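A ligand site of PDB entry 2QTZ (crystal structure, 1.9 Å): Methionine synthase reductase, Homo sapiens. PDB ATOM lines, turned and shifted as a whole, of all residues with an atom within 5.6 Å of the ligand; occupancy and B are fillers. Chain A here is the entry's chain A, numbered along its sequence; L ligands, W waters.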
ATOM      1  N   LYS A 132       2.468  24.698  37.156  1.00  0.00           N
ATOM      2  CA  LYS A 132       3.222  25.897  37.522  1.00  0.00           C
ATOM      3  C   LYS A 132       2.373  27.100  37.173  1.00  0.00           C
ATOM      4  O   LYS A 132       1.729  27.090  36.122  1.00  0.00           O
ATOM      5  CB  LYS A 132       4.538  25.946  36.750  1.00  0.00           C
ATOM      6  CG  LYS A 132       5.404  24.673  36.931  1.00  0.00           C
ATOM      7  CD  LYS A 132       6.843  25.042  36.613  1.00  0.00           C
ATOM      8  CE  LYS A 132       7.310  24.455  35.355  1.00  0.00           C
ATOM      9  NZ  LYS A 132       8.243  23.335  35.706  1.00  0.00           N
ATOM     10  N   ASN A 312       7.201  32.084  35.795  1.00  0.00           N
ATOM     11  CA  ASN A 312       6.591  31.023  36.607  1.00  0.00           C
ATOM     12  C   ASN A 312       6.962  31.291  38.048  1.00  0.00           C
ATOM     13  O   ASN A 312       8.144  31.656  38.359  1.00  0.00           O
ATOM     14  CB  ASN A 312       7.162  29.637  36.224  1.00  0.00           C
ATOM     15  CG  ASN A 312       6.630  29.135  34.911  1.00  0.00           C
ATOM     16  OD1 ASN A 312       5.505  29.456  34.515  1.00  0.00           O
ATOM     17  ND2 ASN A 312       7.432  28.327  34.218  1.00  0.00           N
ATOM     18  N   PRO A 386       9.622  27.253  24.396  1.00  0.00           N
ATOM     19  CA  PRO A 386       8.681  26.449  25.197  1.00  0.00           C
ATOM     20  C   PRO A 386       8.409  27.102  26.540  1.00  0.00           C
ATOM     21  O   PRO A 386       9.306  27.725  27.159  1.00  0.00           O
ATOM     22  CB  PRO A 386       9.407  25.100  25.389  1.00  0.00           C
ATOM     23  CG  PRO A 386      10.836  25.366  25.103  1.00  0.00           C
ATOM     24  CD  PRO A 386      10.973  26.657  24.335  1.00  0.00           C
ATOM     25  N   GLY A 387       7.184  26.941  27.025  1.00  0.00           N
ATOM     26  CA  GLY A 387       6.753  27.580  28.275  1.00  0.00           C
ATOM     27  C   GLY A 387       7.020  29.079  28.324  1.00  0.00           C
ATOM     28  O   GLY A 387       6.770  29.813  27.354  1.00  0.00           O
ATOM     29  N   THR A 388       7.552  29.540  29.454  1.00  0.00           N
ATOM     30  CA  THR A 388       7.783  30.984  29.621  1.00  0.00           C
ATOM     31  C   THR A 388       8.889  31.502  28.730  1.00  0.00           C
ATOM     32  O   THR A 388       9.033  32.724  28.597  1.00  0.00           O
ATOM     33  CB  THR A 388       8.101  31.365  31.057  1.00  0.00           C
ATOM     34  OG1 THR A 388       9.139  30.508  31.500  1.00  0.00           O
ATOM     35  CG2 THR A 388       6.887  31.141  31.968  1.00  0.00           C
ATOM     36  N   GLY A 420       5.858  25.367  22.927  1.00  0.00           N
ATOM     37  CA  GLY A 420       5.545  24.084  23.520  1.00  0.00           C
ATOM     38  C   GLY A 420       4.984  24.351  24.893  1.00  0.00           C
ATOM     39  O   GLY A 420       5.426  25.275  25.576  1.00  0.00           O
ATOM     40  N   CYS A 421       3.987  23.561  25.291  1.00  0.00           N
ATOM     41  CA  CYS A 421       3.532  23.541  26.709  1.00  0.00           C
ATOM     42  C   CYS A 421       3.034  22.144  27.041  1.00  0.00           C
ATOM     43  O   CYS A 421       3.124  21.258  26.208  1.00  0.00           O
ATOM     44  CB  CYS A 421       2.427  24.600  26.952  1.00  0.00           C
ATOM     45  SG  CYS A 421       0.985  24.368  25.939  1.00  0.00           S
ATOM     46  N   ARG A 422       2.543  21.936  28.266  1.00  0.00           N
ATOM     47  CA  ARG A 422       2.096  20.595  28.715  1.00  0.00           C
ATOM     48  C   ARG A 422       0.687  20.252  28.230  1.00  0.00           C
ATOM     49  O   ARG A 422       0.452  19.142  27.772  1.00  0.00           O
ATOM     50  CB  ARG A 422       2.185  20.482  30.237  1.00  0.00           C
ATOM     51  CG  ARG A 422       3.630  20.612  30.772  1.00  0.00           C
ATOM     52  CD  ARG A 422       3.706  20.592  32.284  1.00  0.00           C
ATOM     53  NE  ARG A 422       2.852  21.616  32.867  1.00  0.00           N
ATOM     54  CZ  ARG A 422       3.226  22.870  33.146  1.00  0.00           C
ATOM     55  NH1 ARG A 422       4.496  23.278  32.944  1.00  0.00           N
ATOM     56  NH2 ARG A 422       2.319  23.713  33.653  1.00  0.00           N
ATOM     57  N   ASP A 427      -1.883  25.522  30.057  1.00  0.00           N
ATOM     58  CA  ASP A 427      -0.684  26.381  30.047  1.00  0.00           C
ATOM     59  C   ASP A 427      -0.282  26.823  28.639  1.00  0.00           C
ATOM     60  O   ASP A 427       0.911  27.045  28.362  1.00  0.00           O
ATOM     61  CB  ASP A 427       0.495  25.724  30.778  1.00  0.00           C
ATOM     62  CG  ASP A 427       0.923  24.400  30.148  1.00  0.00           C
ATOM     63  OD1 ASP A 427       0.133  23.828  29.380  1.00  0.00           O
ATOM     64  OD2 ASP A 427       2.072  23.929  30.367  1.00  0.00           O
ATOM     65  N   SER A 449       3.417  22.417  20.318  1.00  0.00           N
ATOM     66  CA  SER A 449       3.436  21.030  20.815  1.00  0.00           C
ATOM     67  C   SER A 449       2.875  20.949  22.229  1.00  0.00           C
ATOM     68  O   SER A 449       3.016  21.888  23.000  1.00  0.00           O
ATOM     69  CB  SER A 449       4.834  20.471  20.742  1.00  0.00           C
ATOM     70  OG  SER A 449       5.719  21.360  21.363  1.00  0.00           O
ATOM     71  N   SER A 451       2.939  18.486  25.449  1.00  0.00           N
ATOM     72  CA  SER A 451       3.762  17.350  25.860  1.00  0.00           C
ATOM     73  C   SER A 451       2.995  16.328  26.674  1.00  0.00           C
ATOM     74  O   SER A 451       3.453  15.172  26.788  1.00  0.00           O
ATOM     75  CB  SER A 451       4.991  17.794  26.627  1.00  0.00           C
ATOM     76  OG  SER A 451       4.598  18.519  27.790  1.00  0.00           O
ATOM     77  N   ARG A 452       1.865  16.732  27.261  1.00  0.00           N
ATOM     78  CA  ARG A 452       1.153  15.791  28.154  1.00  0.00           C
ATOM     79  C   ARG A 452      -0.279  15.546  27.762  1.00  0.00           C
ATOM     80  O   ARG A 452      -1.018  14.930  28.529  1.00  0.00           O
ATOM     81  CB  ARG A 452       1.229  16.245  29.617  1.00  0.00           C
ATOM     82  CG  ARG A 452       2.671  16.435  30.107  1.00  0.00           C
ATOM     83  CD  ARG A 452       2.726  16.799  31.573  1.00  0.00           C
ATOM     84  NE  ARG A 452       4.098  17.167  31.909  1.00  0.00           N
ATOM     85  CZ  ARG A 452       4.590  17.235  33.144  1.00  0.00           C
ATOM     86  NH1 ARG A 452       3.832  16.969  34.206  1.00  0.00           N
ATOM     87  NH2 ARG A 452       5.864  17.598  33.326  1.00  0.00           N
ATOM     88  N   LYS A 464       5.359  16.073  20.582  1.00  0.00           N
ATOM     89  CA  LYS A 464       5.432  16.254  22.029  1.00  0.00           C
ATOM     90  C   LYS A 464       6.193  17.521  22.442  1.00  0.00           C
ATOM     91  O   LYS A 464       5.755  18.273  23.328  1.00  0.00           O
ATOM     92  CB  LYS A 464       6.122  15.052  22.624  1.00  0.00           C
ATOM     93  CG  LYS A 464       6.066  15.003  24.129  1.00  0.00           C
ATOM     94  CD  LYS A 464       7.058  13.962  24.679  1.00  0.00           C
ATOM     95  CE  LYS A 464       7.199  14.086  26.198  1.00  0.00           C
ATOM     96  NZ  LYS A 464       7.759  12.827  26.799  1.00  0.00           N
ATOM     97  N   TYR A 465       7.349  17.746  21.809  1.00  0.00           N
ATOM     98  CA  TYR A 465       8.208  18.888  22.152  1.00  0.00           C
ATOM     99  C   TYR A 465       8.528  19.751  20.922  1.00  0.00           C
ATOM    100  O   TYR A 465       8.335  19.303  19.795  1.00  0.00           O
ATOM    101  CB  TYR A 465       9.540  18.374  22.698  1.00  0.00           C
ATOM    102  CG  TYR A 465       9.502  17.731  24.086  1.00  0.00           C
ATOM    103  CD1 TYR A 465       8.669  18.211  25.096  1.00  0.00           C
ATOM    104  CD2 TYR A 465      10.380  16.707  24.402  1.00  0.00           C
ATOM    105  CE1 TYR A 465       8.660  17.640  26.380  1.00  0.00           C
ATOM    106  CE2 TYR A 465      10.392  16.135  25.699  1.00  0.00           C
ATOM    107  CZ  TYR A 465       9.543  16.613  26.672  1.00  0.00           C
ATOM    108  OH  TYR A 465       9.569  16.035  27.930  1.00  0.00           O
ATOM    109  N   VAL A 466       9.058  20.953  21.145  1.00  0.00           N
ATOM    110  CA  VAL A 466       9.335  21.870  20.029  1.00  0.00           C
ATOM    111  C   VAL A 466      10.292  21.259  18.994  1.00  0.00           C
ATOM    112  O   VAL A 466      10.111  21.460  17.803  1.00  0.00           O
ATOM    113  CB  VAL A 466       9.874  23.240  20.502  1.00  0.00           C
ATOM    114  CG1 VAL A 466       8.721  24.039  21.143  1.00  0.00           C
ATOM    115  CG2 VAL A 466      11.055  23.065  21.456  1.00  0.00           C
ATOM    116  N   GLN A 467      11.268  20.486  19.427  1.00  0.00           N
ATOM    117  CA  GLN A 467      12.244  19.908  18.458  1.00  0.00           C
ATOM    118  C   GLN A 467      11.578  18.914  17.484  1.00  0.00           C
ATOM    119  O   GLN A 467      12.020  18.756  16.333  1.00  0.00           O
ATOM    120  CB  GLN A 467      13.434  19.255  19.161  1.00  0.00           C
ATOM    121  CG  GLN A 467      13.058  18.204  20.186  1.00  0.00           C
ATOM    122  CD  GLN A 467      12.918  18.770  21.596  1.00  0.00           C
ATOM    123  OE1 GLN A 467      12.603  19.935  21.790  1.00  0.00           O
ATOM    124  NE2 GLN A 467      13.174  17.937  22.581  1.00  0.00           N
ATOM    125  N   ASP A 493      13.983  27.932  30.037  1.00  0.00           N
ATOM    126  CA  ASP A 493      14.670  27.690  31.313  1.00  0.00           C
ATOM    127  C   ASP A 493      15.664  26.528  31.266  1.00  0.00           C
ATOM    128  O   ASP A 493      16.699  26.606  31.954  1.00  0.00           O
ATOM    129  CB  ASP A 493      13.698  27.612  32.514  1.00  0.00           C
ATOM    130  CG  ASP A 493      14.421  27.666  33.855  1.00  0.00           C
ATOM    131  OD1 ASP A 493      15.340  28.509  34.014  1.00  0.00           O
ATOM    132  OD2 ASP A 493      14.072  26.873  34.777  1.00  0.00           O
ATOM    133  N   ALA A 494      15.381  25.482  30.476  1.00  0.00           N
ATOM    134  CA  ALA A 494      16.201  24.236  30.468  1.00  0.00           C
ATOM    135  C   ALA A 494      17.386  24.257  29.494  1.00  0.00           C
ATOM    136  O   ALA A 494      17.225  24.576  28.287  1.00  0.00           O
ATOM    137  CB  ALA A 494      15.300  22.999  30.192  1.00  0.00           C
ATOM    138  N   ASN A 496      18.734  21.432  28.913  1.00  0.00           N
ATOM    139  CA  ASN A 496      18.282  20.242  28.217  1.00  0.00           C
ATOM    140  C   ASN A 496      17.520  20.580  26.947  1.00  0.00           C
ATOM    141  O   ASN A 496      17.797  20.011  25.926  1.00  0.00           O
ATOM    142  CB  ASN A 496      17.428  19.330  29.095  1.00  0.00           C
ATOM    143  CG  ASN A 496      18.221  18.151  29.686  1.00  0.00           C
ATOM    144  OD1 ASN A 496      17.643  17.099  30.012  1.00  0.00           O
ATOM    145  ND2 ASN A 496      19.531  18.321  29.842  1.00  0.00           N
ATOM    146  N   MET A 497      16.553  21.500  27.039  1.00  0.00           N
ATOM    147  CA  MET A 497      15.803  21.910  25.859  1.00  0.00           C
ATOM    148  C   MET A 497      16.741  22.479  24.798  1.00  0.00           C
ATOM    149  O   MET A 497      16.640  22.116  23.637  1.00  0.00           O
ATOM    150  CB  MET A 497      14.674  22.893  26.237  1.00  0.00           C
ATOM    151  CG  MET A 497      13.825  23.344  25.066  1.00  0.00           C
ATOM    152  SD  MET A 497      14.551  24.768  24.226  1.00  0.00           S
ATOM    153  CE  MET A 497      14.574  25.984  25.593  1.00  0.00           C
ATOM    154  N   ASP A 500      18.681  19.677  23.111  1.00  0.00           N
ATOM    155  CA  ASP A 500      17.790  18.907  22.257  1.00  0.00           C
ATOM    156  C   ASP A 500      17.425  19.641  20.965  1.00  0.00           C
ATOM    157  O   ASP A 500      17.284  19.037  19.911  1.00  0.00           O
ATOM    158  CB  ASP A 500      16.519  18.521  23.005  1.00  0.00           C
ATOM    159  CG  ASP A 500      16.781  17.500  24.108  1.00  0.00           C
ATOM    160  OD1 ASP A 500      17.828  16.820  24.077  1.00  0.00           O
ATOM    161  OD2 ASP A 500      15.945  17.390  25.021  1.00  0.00           O
HETATM  162  P1  LIG L   1       8.848  24.049  31.686  1.00  0.00           P
HETATM  163  O1  LIG L   1       8.047  25.308  31.838  1.00  0.00           O
HETATM  164  O2  LIG L   1       8.553  23.143  32.809  1.00  0.00           O
HETATM  165  O3  LIG L   1       8.587  23.383  30.251  1.00  0.00           O
HETATM  166  C1  LIG L   1       7.668  23.915  29.303  1.00  0.00           C
HETATM  167  C2  LIG L   1       7.466  22.929  28.156  1.00  0.00           C
HETATM  168  O4  LIG L   1       8.723  22.445  27.692  1.00  0.00           O
HETATM  169  C3  LIG L   1       6.683  21.725  28.658  1.00  0.00           C
HETATM  170  O5  LIG L   1       5.910  21.154  27.641  1.00  0.00           O
HETATM  171  C4  LIG L   1       7.744  20.694  28.969  1.00  0.00           C
HETATM  172  O6  LIG L   1       7.167  19.413  28.825  1.00  0.00           O
HETATM  173  C5  LIG L   1       8.735  21.028  27.843  1.00  0.00           C
HETATM  174  N1  LIG L   1      10.069  20.367  27.947  1.00  0.00           N
HETATM  175  C6  LIG L   1      10.648  19.691  29.010  1.00  0.00           C
HETATM  176  N2  LIG L   1      11.853  19.196  28.592  1.00  0.00           N
HETATM  177  C7  LIG L   1      12.043  19.529  27.274  1.00  0.00           C
HETATM  178  C8  LIG L   1      13.070  19.301  26.350  1.00  0.00           C
HETATM  179  N3  LIG L   1      14.191  18.622  26.669  1.00  0.00           N
HETATM  180  N4  LIG L   1      12.946  19.802  25.073  1.00  0.00           N
HETATM  181  C9  LIG L   1      11.823  20.518  24.698  1.00  0.00           C
HETATM  182  N5  LIG L   1      10.822  20.756  25.609  1.00  0.00           N
HETATM  183  C10 LIG L   1      10.931  20.271  26.881  1.00  0.00           C
HETATM  184  O7  LIG L   1      10.414  24.359  31.753  1.00  0.00           O
HETATM  185  P2  LIG L   1      11.434  23.791  32.877  1.00  0.00           P
HETATM  186  O8  LIG L   1      10.737  24.141  34.283  1.00  0.00           O
HETATM  187  O9  LIG L   1      12.677  24.596  32.807  1.00  0.00           O
HETATM  188  O10 LIG L   1      11.475  22.309  32.778  1.00  0.00           O
HETATM  189  P3  LIG L   1       7.228  18.311  30.032  1.00  0.00           P
HETATM  190  O11 LIG L   1       8.461  17.503  29.795  1.00  0.00           O
HETATM  191  O12 LIG L   1       5.984  17.467  29.863  1.00  0.00           O
HETATM  192  O13 LIG L   1       7.299  19.105  31.325  1.00  0.00           O
HETATM  193  O   HOH W   1       9.950  18.991  32.720  1.00  0.00           O
HETATM  194  O   HOH W   2       4.512  24.819  29.883  1.00  0.00           O
HETATM  195  O   HOH W   3      12.031  23.161  28.180  1.00  0.00           O
HETATM  196  O   HOH W   4       5.988  20.869  24.370  1.00  0.00           O
HETATM  197  O   HOH W   5       6.612  21.469  32.503  1.00  0.00           O
HETATM  198  O   HOH W   6       8.693  21.738  23.967  1.00  0.00           O
HETATM  199  O   HOH W   7       6.487  15.105  29.982  1.00  0.00           O
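The side-chain hydroxyl of Ser 451 lies within hydrogen-bond range of an oxygen (O12) of the ligand (2.7 Å). The side-chain amino group (NZ) of Lys 132 lies within salt-bridge range of an oxygen (O2) of the ligand. The side-chain hydroxyl of Tyr 465 lies within hydrogen-bond range of an oxygen (O11) of the ligand (2.6 Å). The side-chain carboxylate (OD2) of Asp 500 is in hydrogen-bond range of a nitrogen (N3) of the ligand, 2.7 Å away. O of Cys 421 lies close to O5 of the ligand, 3.1 Å away. The guanidinium group of Arg 452 is in salt-bridge range of an oxygen (O12) of the ligand (2.8 Å). The side-chain amide nitrogen (NE2) of Gln 467 is in hydrogen-bond range of a nitrogen (N4) of the ligand, 3.1 Å away.
The guanidinium group (NH2) of Arg 422 lies within salt-bridge range of the side-chain carboxylate (OD2) of Asp 427 (3.3 Å). The side-chain sulfur (SG) of Cys 421 sits close to the side-chain carboxylate (OD1) of Asp 427 (3.6 Å). The backbone NH of Arg 452 is in hydrogen-bond range of the backbone carbonyl oxygen of Arg 422. O of Gly 420 is in hydrogen-bond range of N of Gly 387. The backbone carbonyl oxygen (O) of Ser 449 sits at hydrogen-bond distance from the backbone NH (N) of Cys 421, 3.0 Å away. The backbone NH (N) of Ser 451 sits at hydrogen-bond distance from the backbone carbonyl oxygen (O) of Cys 421 (2.9 Å). N of Ser 451 sits at hydrogen-bond distance from O of Arg 422 (3.5 Å).
O9 of the ligand sits close to OD2 of Asp 493, 3.3 Å away. Merely in contact with the ligand: Asn 312 (3.9 Å), Pro 386 (3.6 Å), Gly 387 (3.8 Å), Arg 422 (3.5 Å), Ala 494 (3.7 Å), Asn 496 (3.9 Å) and Met 497 (3.5 Å). Hydrophobic or aromatic side chains within 4 Å of the ligand: Pro 386, Tyr 465 and Met 497. 15 residues have an atom within 4 Å of the ligand: Lys 132, Asn 312, Pro 386, Gly 387, Cys 421, Arg 422, Ser 451, Arg 452, Tyr 465, Gln 467, Asp 493, Ala 494, Asn 496, Met 497 and Asp 500. The nearest printed residue that does not touch the ligand is Gly 420 (4.04 Å).
Water W5 bridges O2 of the ligand (2.6 Å) and NH1 of Arg 422 (2.8 Å). Water W6 bridges a nitrogen (N5) of the ligand and the backbone NH (N) of Val 466. Water W4 lies within hydrogen-bond range of the backbone carbonyl oxygen (O) of Lys 464 (2.8 Å), the side-chain hydroxyl (OG) of Ser 449 (3.1 Å), an oxygen (O5) of the ligand (3.3 Å) and the backbone carbonyl oxygen (O) of Cys 421 (3.4 Å). Water W2 lies within hydrogen-bond range of the side-chain carboxylate (OD2) of Asp 427 and the guanidinium group (NH1) of Arg 422.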
